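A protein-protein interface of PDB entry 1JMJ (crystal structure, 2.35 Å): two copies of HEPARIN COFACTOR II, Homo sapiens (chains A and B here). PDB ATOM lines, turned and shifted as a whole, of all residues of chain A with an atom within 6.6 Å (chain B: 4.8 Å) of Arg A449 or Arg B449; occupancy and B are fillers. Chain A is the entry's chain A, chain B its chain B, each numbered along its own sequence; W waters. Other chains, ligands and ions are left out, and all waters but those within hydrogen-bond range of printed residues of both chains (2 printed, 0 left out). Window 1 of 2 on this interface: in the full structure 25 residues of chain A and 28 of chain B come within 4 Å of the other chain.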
ATOM      1  N   PHE A  67       3.700  28.113 -31.914  1.00  0.00           N
ATOM      2  CA  PHE A  67       2.782  28.727 -30.969  1.00  0.00           C
ATOM      3  C   PHE A  67       2.584  27.761 -29.805  1.00  0.00           C
ATOM      4  O   PHE A  67       2.416  28.179 -28.662  1.00  0.00           O
ATOM      5  CB  PHE A  67       1.435  29.011 -31.631  1.00  0.00           C
ATOM      6  CG  PHE A  67       0.537  29.888 -30.809  1.00  0.00           C
ATOM      7  CD1 PHE A  67       0.798  31.249 -30.689  1.00  0.00           C
ATOM      8  CD2 PHE A  67      -0.561  29.354 -30.142  1.00  0.00           C
ATOM      9  CE1 PHE A  67      -0.021  32.067 -29.917  1.00  0.00           C
ATOM     10  CE2 PHE A  67      -1.385  30.162 -29.367  1.00  0.00           C
ATOM     11  CZ  PHE A  67      -1.117  31.520 -29.254  1.00  0.00           C
ATOM     12  N   GLU A  69       3.263  25.123 -26.839  1.00  0.00           N
ATOM     13  CA  GLU A  69       4.240  25.165 -25.759  1.00  0.00           C
ATOM     14  C   GLU A  69       4.823  23.790 -25.438  1.00  0.00           C
ATOM     15  O   GLU A  69       5.131  23.500 -24.283  1.00  0.00           O
ATOM     16  CB  GLU A  69       3.588  25.753 -24.504  1.00  0.00           C
ATOM     17  CG  GLU A  69       2.410  24.937 -23.998  1.00  0.00           C
ATOM     18  CD  GLU A  69       1.708  25.576 -22.819  1.00  0.00           C
ATOM     19  OE1 GLU A  69       1.023  26.603 -23.011  1.00  0.00           O
ATOM     20  OE2 GLU A  69       1.845  25.049 -21.696  1.00  0.00           O
ATOM     21  N   HIS A 292       3.500  16.901 -20.371  1.00  0.00           N
ATOM     22  CA  HIS A 292       3.171  18.315 -20.285  1.00  0.00           C
ATOM     23  C   HIS A 292       3.599  18.755 -18.894  1.00  0.00           C
ATOM     24  O   HIS A 292       3.516  17.974 -17.945  1.00  0.00           O
ATOM     25  CB  HIS A 292       1.663  18.479 -20.459  1.00  0.00           C
ATOM     26  CG  HIS A 292       1.204  19.899 -20.548  1.00  0.00           C
ATOM     27  ND1 HIS A 292       0.760  20.463 -21.724  1.00  0.00           N
ATOM     28  CD2 HIS A 292       1.088  20.862 -19.604  1.00  0.00           C
ATOM     29  CE1 HIS A 292       0.388  21.711 -21.502  1.00  0.00           C
ATOM     30  NE2 HIS A 292       0.577  21.979 -20.223  1.00  0.00           N
ATOM     31  N   LYS A 310     -11.720  16.778 -26.459  1.00  0.00           N
ATOM     32  CA  LYS A 310     -12.621  17.872 -26.805  1.00  0.00           C
ATOM     33  C   LYS A 310     -14.051  17.388 -26.531  1.00  0.00           C
ATOM     34  O   LYS A 310     -14.335  16.200 -26.667  1.00  0.00           O
ATOM     35  CB  LYS A 310     -12.483  18.236 -28.279  1.00  0.00           C
ATOM     36  CG  LYS A 310     -11.089  18.630 -28.702  1.00  0.00           C
ATOM     37  CD  LYS A 310     -11.097  19.007 -30.166  1.00  0.00           C
ATOM     38  CE  LYS A 310      -9.722  19.380 -30.668  1.00  0.00           C
ATOM     39  NZ  LYS A 310      -9.729  19.503 -32.153  1.00  0.00           N
ATOM     40  N   THR A 370     -18.219  24.239 -25.452  1.00  0.00           N
ATOM     41  CA  THR A 370     -17.427  23.205 -26.121  1.00  0.00           C
ATOM     42  C   THR A 370     -15.986  23.508 -25.691  1.00  0.00           C
ATOM     43  O   THR A 370     -15.421  24.566 -26.013  1.00  0.00           O
ATOM     44  CB  THR A 370     -17.569  23.259 -27.657  1.00  0.00           C
ATOM     45  OG1 THR A 370     -18.883  22.830 -28.026  1.00  0.00           O
ATOM     46  CG2 THR A 370     -16.576  22.327 -28.309  1.00  0.00           C
ATOM     47  N   ARG A 371     -15.401  22.578 -24.944  1.00  0.00           N
ATOM     48  CA  ARG A 371     -14.072  22.788 -24.400  1.00  0.00           C
ATOM     49  C   ARG A 371     -13.036  21.746 -24.731  1.00  0.00           C
ATOM     50  O   ARG A 371     -13.321  20.548 -24.762  1.00  0.00           O
ATOM     51  CB  ARG A 371     -14.137  22.864 -22.865  1.00  0.00           C
ATOM     52  CG  ARG A 371     -15.254  23.696 -22.272  1.00  0.00           C
ATOM     53  CD  ARG A 371     -15.314  23.489 -20.773  1.00  0.00           C
ATOM     54  NE  ARG A 371     -16.543  24.036 -20.212  1.00  0.00           N
ATOM     55  CZ  ARG A 371     -16.742  25.325 -19.977  1.00  0.00           C
ATOM     56  NH1 ARG A 371     -17.902  25.733 -19.482  1.00  0.00           N
ATOM     57  NH2 ARG A 371     -15.776  26.202 -20.212  1.00  0.00           N
ATOM     58  N   GLU A 372     -11.819  22.227 -24.958  1.00  0.00           N
ATOM     59  CA  GLU A 372     -10.682  21.358 -25.191  1.00  0.00           C
ATOM     60  C   GLU A 372     -10.224  21.204 -23.740  1.00  0.00           C
ATOM     61  O   GLU A 372     -10.042  22.204 -23.032  1.00  0.00           O
ATOM     62  CB  GLU A 372      -9.619  22.076 -26.016  1.00  0.00           C
ATOM     63  CG  GLU A 372      -8.334  21.277 -26.209  1.00  0.00           C
ATOM     64  CD  GLU A 372      -7.320  22.013 -27.077  1.00  0.00           C
ATOM     65  OE1 GLU A 372      -6.168  21.537 -27.200  1.00  0.00           O
ATOM     66  OE2 GLU A 372      -7.680  23.069 -27.639  1.00  0.00           O
ATOM     67  N   VAL A 373     -10.070  19.968 -23.279  1.00  0.00           N
ATOM     68  CA  VAL A 373      -9.679  19.746 -21.894  1.00  0.00           C
ATOM     69  C   VAL A 373      -8.442  18.889 -21.734  1.00  0.00           C
ATOM     70  O   VAL A 373      -8.361  17.792 -22.285  1.00  0.00           O
ATOM     71  CB  VAL A 373     -10.831  19.080 -21.092  1.00  0.00           C
ATOM     72  CG1 VAL A 373     -10.354  18.696 -19.705  1.00  0.00           C
ATOM     73  CG2 VAL A 373     -12.005  20.024 -20.994  1.00  0.00           C
ATOM     74  N   LEU A 374      -7.472  19.402 -20.984  1.00  0.00           N
ATOM     75  CA  LEU A 374      -6.254  18.657 -20.708  1.00  0.00           C
ATOM     76  C   LEU A 374      -6.244  18.313 -19.230  1.00  0.00           C
ATOM     77  O   LEU A 374      -6.310  19.191 -18.364  1.00  0.00           O
ATOM     78  CB  LEU A 374      -5.004  19.462 -21.062  1.00  0.00           C
ATOM     79  CG  LEU A 374      -4.677  19.501 -22.551  1.00  0.00           C
ATOM     80  CD1 LEU A 374      -5.762  20.307 -23.281  1.00  0.00           C
ATOM     81  CD2 LEU A 374      -3.303  20.120 -22.755  1.00  0.00           C
ATOM     82  N   SER A 445     -14.434  21.532 -33.671  1.00  0.00           N
ATOM     83  CA  SER A 445     -13.840  22.729 -33.079  1.00  0.00           C
ATOM     84  C   SER A 445     -14.342  22.951 -31.662  1.00  0.00           C
ATOM     85  O   SER A 445     -15.373  22.402 -31.278  1.00  0.00           O
ATOM     86  CB  SER A 445     -14.163  23.970 -33.912  1.00  0.00           C
ATOM     87  OG  SER A 445     -15.450  24.469 -33.589  1.00  0.00           O
ATOM     88  N   THR A 446     -13.602  23.751 -30.893  1.00  0.00           N
ATOM     89  CA  THR A 446     -13.970  24.077 -29.512  1.00  0.00           C
ATOM     90  C   THR A 446     -13.719  25.561 -29.258  1.00  0.00           C
ATOM     91  O   THR A 446     -12.685  26.102 -29.657  1.00  0.00           O
ATOM     92  CB  THR A 446     -13.159  23.252 -28.490  1.00  0.00           C
ATOM     93  OG1 THR A 446     -11.763  23.490 -28.681  1.00  0.00           O
ATOM     94  CG2 THR A 446     -13.440  21.763 -28.658  1.00  0.00           C
ATOM     95  N   GLN A 447     -14.670  26.217 -28.601  1.00  0.00           N
ATOM     96  CA  GLN A 447     -14.568  27.644 -28.320  1.00  0.00           C
ATOM     97  C   GLN A 447     -13.579  27.995 -27.210  1.00  0.00           C
ATOM     98  O   GLN A 447     -13.058  29.114 -27.164  1.00  0.00           O
ATOM     99  CB  GLN A 447     -15.950  28.203 -27.965  1.00  0.00           C
ATOM    100  CG  GLN A 447     -15.925  29.625 -27.411  1.00  0.00           C
ATOM    101  CD  GLN A 447     -17.302  30.130 -27.047  1.00  0.00           C
ATOM    102  OE1 GLN A 447     -18.121  29.394 -26.500  1.00  0.00           O
ATOM    103  NE2 GLN A 447     -17.565  31.396 -27.342  1.00  0.00           N
ATOM    104  N   VAL A 448     -13.327  27.049 -26.310  1.00  0.00           N
ATOM    105  CA  VAL A 448     -12.398  27.305 -25.218  1.00  0.00           C
ATOM    106  C   VAL A 448     -11.536  26.099 -24.894  1.00  0.00           C
ATOM    107  O   VAL A 448     -11.726  25.008 -25.443  1.00  0.00           O
ATOM    108  CB  VAL A 448     -13.131  27.732 -23.924  1.00  0.00           C
ATOM    109  CG1 VAL A 448     -14.050  28.896 -24.223  1.00  0.00           C
ATOM    110  CG2 VAL A 448     -13.909  26.558 -23.341  1.00  0.00           C
ATOM    111  N   ARG A 449     -10.586  26.313 -23.991  1.00  0.00           N
ATOM    112  CA  ARG A 449      -9.677  25.265 -23.565  1.00  0.00           C
ATOM    113  C   ARG A 449      -9.295  25.484 -22.105  1.00  0.00           C
ATOM    114  O   ARG A 449      -9.159  26.630 -21.652  1.00  0.00           O
ATOM    115  CB  ARG A 449      -8.414  25.279 -24.433  1.00  0.00           C
ATOM    116  CG  ARG A 449      -7.520  24.062 -24.264  1.00  0.00           C
ATOM    117  CD  ARG A 449      -6.200  24.410 -23.629  1.00  0.00           C
ATOM    118  NE  ARG A 449      -5.509  25.497 -24.325  1.00  0.00           N
ATOM    119  CZ  ARG A 449      -4.633  26.308 -23.730  1.00  0.00           C
ATOM    120  NH1 ARG A 449      -4.351  26.142 -22.442  1.00  0.00           N
ATOM    121  NH2 ARG A 449      -4.066  27.302 -24.401  1.00  0.00           N
ATOM    122  N   PHE A 450      -9.161  24.391 -21.361  1.00  0.00           N
ATOM    123  CA  PHE A 450      -8.743  24.492 -19.975  1.00  0.00           C
ATOM    124  C   PHE A 450      -7.717  23.419 -19.686  1.00  0.00           C
ATOM    125  O   PHE A 450      -7.985  22.218 -19.840  1.00  0.00           O
ATOM    126  CB  PHE A 450      -9.903  24.336 -18.995  1.00  0.00           C
ATOM    127  CG  PHE A 450      -9.528  24.693 -17.581  1.00  0.00           C
ATOM    128  CD1 PHE A 450      -9.344  26.024 -17.215  1.00  0.00           C
ATOM    129  CD2 PHE A 450      -9.287  23.703 -16.635  1.00  0.00           C
ATOM    130  CE1 PHE A 450      -8.920  26.363 -15.927  1.00  0.00           C
ATOM    131  CE2 PHE A 450      -8.862  24.034 -15.347  1.00  0.00           C
ATOM    132  CZ  PHE A 450      -8.678  25.369 -14.996  1.00  0.00           C
ATOM    133  N   THR A 451      -6.539  23.862 -19.265  1.00  0.00           N
ATOM    134  CA  THR A 451      -5.462  22.957 -18.943  1.00  0.00           C
ATOM    135  C   THR A 451      -5.270  22.856 -17.437  1.00  0.00           C
ATOM    136  O   THR A 451      -5.022  23.858 -16.763  1.00  0.00           O
ATOM    137  CB  THR A 451      -4.150  23.425 -19.577  1.00  0.00           C
ATOM    138  OG1 THR A 451      -4.312  23.473 -21.002  1.00  0.00           O
ATOM    139  CG2 THR A 451      -2.996  22.482 -19.197  1.00  0.00           C
ATOM    140  N   GLU B 372      -4.722  32.090 -23.979  1.00  0.00           N
ATOM    141  CA  GLU B 372      -4.446  32.098 -25.408  1.00  0.00           C
ATOM    142  C   GLU B 372      -5.738  32.760 -25.877  1.00  0.00           C
ATOM    143  O   GLU B 372      -6.835  32.264 -25.570  1.00  0.00           O
ATOM    144  CB  GLU B 372      -4.365  30.679 -25.964  1.00  0.00           C
ATOM    145  CG  GLU B 372      -4.235  30.629 -27.475  1.00  0.00           C
ATOM    146  CD  GLU B 372      -4.153  29.213 -28.014  1.00  0.00           C
ATOM    147  OE1 GLU B 372      -4.068  29.048 -29.251  1.00  0.00           O
ATOM    148  OE2 GLU B 372      -4.174  28.260 -27.209  1.00  0.00           O
ATOM    149  N   LEU B 374      -7.996  34.257 -29.116  1.00  0.00           N
ATOM    150  CA  LEU B 374      -8.200  34.426 -30.544  1.00  0.00           C
ATOM    151  C   LEU B 374      -9.275  35.491 -30.736  1.00  0.00           C
ATOM    152  O   LEU B 374     -10.381  35.377 -30.210  1.00  0.00           O
ATOM    153  CB  LEU B 374      -8.610  33.108 -31.208  1.00  0.00           C
ATOM    154  CG  LEU B 374      -7.467  32.102 -31.376  1.00  0.00           C
ATOM    155  CD1 LEU B 374      -7.125  31.477 -30.035  1.00  0.00           C
ATOM    156  CD2 LEU B 374      -7.873  31.029 -32.384  1.00  0.00           C
ATOM    157  N   THR B 446       0.009  28.978 -21.433  1.00  0.00           N
ATOM    158  CA  THR B 446      -1.264  29.529 -21.009  1.00  0.00           C
ATOM    159  C   THR B 446      -2.108  28.407 -20.432  1.00  0.00           C
ATOM    160  O   THR B 446      -2.070  27.275 -20.913  1.00  0.00           O
ATOM    161  CB  THR B 446      -2.010  30.178 -22.178  1.00  0.00           C
ATOM    162  OG1 THR B 446      -2.171  29.225 -23.240  1.00  0.00           O
ATOM    163  CG2 THR B 446      -1.234  31.392 -22.678  1.00  0.00           C
ATOM    164  N   GLN B 447      -2.866  28.736 -19.395  1.00  0.00           N
ATOM    165  CA  GLN B 447      -3.714  27.770 -18.722  1.00  0.00           C
ATOM    166  C   GLN B 447      -5.053  27.577 -19.418  1.00  0.00           C
ATOM    167  O   GLN B 447      -5.648  26.498 -19.334  1.00  0.00           O
ATOM    168  CB  GLN B 447      -3.944  28.212 -17.275  1.00  0.00           C
ATOM    169  CG  GLN B 447      -5.010  27.416 -16.552  1.00  0.00           C
ATOM    170  CD  GLN B 447      -5.100  27.748 -15.080  1.00  0.00           C
ATOM    171  OE1 GLN B 447      -4.968  28.905 -14.679  1.00  0.00           O
ATOM    172  NE2 GLN B 447      -5.340  26.731 -14.263  1.00  0.00           N
ATOM    173  N   VAL B 448      -5.524  28.621 -20.100  1.00  0.00           N
ATOM    174  CA  VAL B 448      -6.812  28.565 -20.788  1.00  0.00           C
ATOM    175  C   VAL B 448      -6.795  29.269 -22.138  1.00  0.00           C
ATOM    176  O   VAL B 448      -5.887  30.047 -22.427  1.00  0.00           O
ATOM    177  CB  VAL B 448      -7.922  29.214 -19.936  1.00  0.00           C
ATOM    178  CG1 VAL B 448      -7.839  28.709 -18.520  1.00  0.00           C
ATOM    179  CG2 VAL B 448      -7.801  30.716 -19.970  1.00  0.00           C
ATOM    180  N   ARG B 449      -7.804  28.988 -22.957  1.00  0.00           N
ATOM    181  CA  ARG B 449      -7.921  29.613 -24.271  1.00  0.00           C
ATOM    182  C   ARG B 449      -9.348  30.088 -24.478  1.00  0.00           C
ATOM    183  O   ARG B 449     -10.293  29.473 -23.988  1.00  0.00           O
ATOM    184  CB  ARG B 449      -7.575  28.630 -25.391  1.00  0.00           C
ATOM    185  CG  ARG B 449      -7.357  29.301 -26.745  1.00  0.00           C
ATOM    186  CD  ARG B 449      -8.285  28.800 -27.836  1.00  0.00           C
ATOM    187  NE  ARG B 449      -8.356  27.344 -27.894  1.00  0.00           N
ATOM    188  CZ  ARG B 449      -9.473  26.675 -28.172  1.00  0.00           C
ATOM    189  NH1 ARG B 449     -10.595  27.332 -28.429  1.00  0.00           N
ATOM    190  NH2 ARG B 449      -9.485  25.353 -28.145  1.00  0.00           N
ATOM    191  N   PHE B 450      -9.498  31.196 -25.190  1.00  0.00           N
ATOM    192  CA  PHE B 450     -10.819  31.712 -25.492  1.00  0.00           C
ATOM    193  C   PHE B 450     -10.846  32.230 -26.922  1.00  0.00           C
ATOM    194  O   PHE B 450     -10.130  33.179 -27.283  1.00  0.00           O
ATOM    195  CB  PHE B 450     -11.238  32.838 -24.545  1.00  0.00           C
ATOM    196  CG  PHE B 450     -12.695  33.168 -24.648  1.00  0.00           C
ATOM    197  CD1 PHE B 450     -13.648  32.364 -24.022  1.00  0.00           C
ATOM    198  CD2 PHE B 450     -13.128  34.202 -25.463  1.00  0.00           C
ATOM    199  CE1 PHE B 450     -15.006  32.581 -24.212  1.00  0.00           C
ATOM    200  CE2 PHE B 450     -14.490  34.427 -25.661  1.00  0.00           C
ATOM    201  CZ  PHE B 450     -15.428  33.611 -25.033  1.00  0.00           C
ATOM    202  N   THR B 451     -11.672  31.586 -27.738  1.00  0.00           N
ATOM    203  CA  THR B 451     -11.812  31.953 -29.129  1.00  0.00           C
ATOM    204  C   THR B 451     -13.085  32.748 -29.316  1.00  0.00           C
ATOM    205  O   THR B 451     -14.162  32.301 -28.918  1.00  0.00           O
ATOM    206  CB  THR B 451     -11.896  30.711 -30.005  1.00  0.00           C
ATOM    207  OG1 THR B 451     -10.742  29.893 -29.776  1.00  0.00           O
ATOM    208  CG2 THR B 451     -11.975  31.100 -31.472  1.00  0.00           C
HETATM  209  O   HOH W   1      -6.153  26.126 -27.356  1.00  0.00           O
HETATM  210  O   HOH W   2       0.062  28.286 -24.652  1.00  0.00           O
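The backbone NH of Thr B446 lies within hydrogen-bond range of the side-chain carboxylate of Glu A69 (3.0 Å).
OE2 of Glu A372 lies within salt-bridge range of NH2 of Arg B449 (3.0 Å).
The backbone carbonyl oxygen of Thr A446 sits at hydrogen-bond distance from the guanidinium group of Arg B449.
O of Gln A447 lies close to NH1 of Arg B449.
The backbone carbonyl oxygen (O) of Gln A447 is in hydrogen-bond range of the backbone NH (N) of Thr B451, at 2.9 Å.
NH2 of Arg A449 is in salt-bridge range of OE2 of Glu B372 (3.0 Å).
The guanidinium group (NH2) of Arg A449 sits at hydrogen-bond distance from the side-chain hydroxyl (OG1) of Thr B446, 2.9 Å away.
O of Gln B447 is in hydrogen-bond range of NH1 of Arg A449, 3.4 Å away.
O of Arg A449 lies within hydrogen-bond range of N of Arg B449 (3.0 Å).
The backbone NH of Thr A451 is in hydrogen-bond range of the backbone carbonyl oxygen of Gln B447 (2.8 Å).
N of Val A448 lies close to NH1 of Arg B449 (3.5 Å).
N of Gln A447 is in hydrogen-bond range of O of Thr A370.
O of Val A448 sits at hydrogen-bond distance from N of Glu A372 (2.8 Å).
The backbone carbonyl oxygen of Glu A372 sits at hydrogen-bond distance from the backbone NH of Phe A450.
The backbone carbonyl oxygen (O) of Phe A450 sits at hydrogen-bond distance from the backbone NH (N) of Leu A374 (3.1 Å).
The guanidinium group (NH1) of Arg A449 lies within hydrogen-bond range of the side-chain hydroxyl (OG1) of Thr A451 (3.0 Å).
The guanidinium group of Arg B449 sits at hydrogen-bond distance from the side-chain hydroxyl of Thr B451 (2.9 Å).
CE2 of Phe A67 touches OE1 of Glu B372 (2.9 Å).
Gln A447 touches Phe B450.
CG1 of Val A448 touches CD1 of Phe B450, 3.5 Å away.
Arg A449 touches Val B448 (O to CA, 3.2 Å).
Gln B447 touches Phe A450.
CG1 of Val B448 touches CD1 of Phe A450, 3.3 Å away.
Of chain B, only Glu B372, Thr B446, Gln B447, Val B448 and Arg B449 come within 4 Å of Arg A449.
Arg B449 touches just these residues of chain A: Glu A372 (3.0 Å), Thr A446 (2.7 Å), Gln A447 (3.3 Å), Val A448 (3.3 Å) and Arg A449 (3.0 Å).
Printed residues of chain B within 4 Å of Glu A372: Arg B449.
Of the printed residues of chain B, Phe A450 touches Gln B447 (3.7 Å) and Val B448 (3.3 Å).
Of the printed residues of chain A, Gln B447 touches Arg A449 (3.4 Å), Phe A450 (3.7 Å) and Thr A451 (2.8 Å).
Of the printed residues of chain A, Val B448 touches Arg A449 (3.2 Å) and Phe A450 (3.3 Å).
Ser A445 touches none of the printed residues of chain B.
Hydrophobic or aromatic side chains of chain B within 4 Å of the printed part of chain A: Val B448 and Phe B450.
Printed residues of chain A that touch a printed residue of chain B: Phe A67, Glu A69, Glu A372, Thr A446, Gln A447, Val A448, Arg A449, Phe A450 and Thr A451.
Hydrophobic or aromatic side chains of chain A within 4 Å of the printed part of chain B: Phe A67, Val A448 and Phe A450.
Along chain A the printed residues that touch a printed residue of chain B span positions 67 to 451.
Among the printed residues, Asp or Glu carboxylates within 4 Å of a Lys or Arg side-chain nitrogen of the other chain: Glu A372 with Arg B449 (3.0 Å) and Arg A449 with Glu B372 (3.0 Å).
Glu A372 touches Arg B449, and with the chains exchanged Arg A449 touches Glu B372.
Gln A447 touches Phe B450, and with the chains exchanged Phe A450 touches Gln B447.
Val A448 touches Phe B450, and with the chains exchanged Phe A450 touches Val B448.
Arg A449 touches its own counterpart, Arg B449.
8 positions are printed for both chains.
Water W2 lies within hydrogen-bond range of OE1 of Glu A69 (2.5 Å) and OG1 of Thr B446 (2.8 Å).
Water W1 lies within hydrogen-bond range of NE of Arg B449 (2.6 Å), OE2 of Glu B372 (2.9 Å), NE of Arg A449 (3.2 Å) and OE2 of Glu A372 (3.4 Å).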
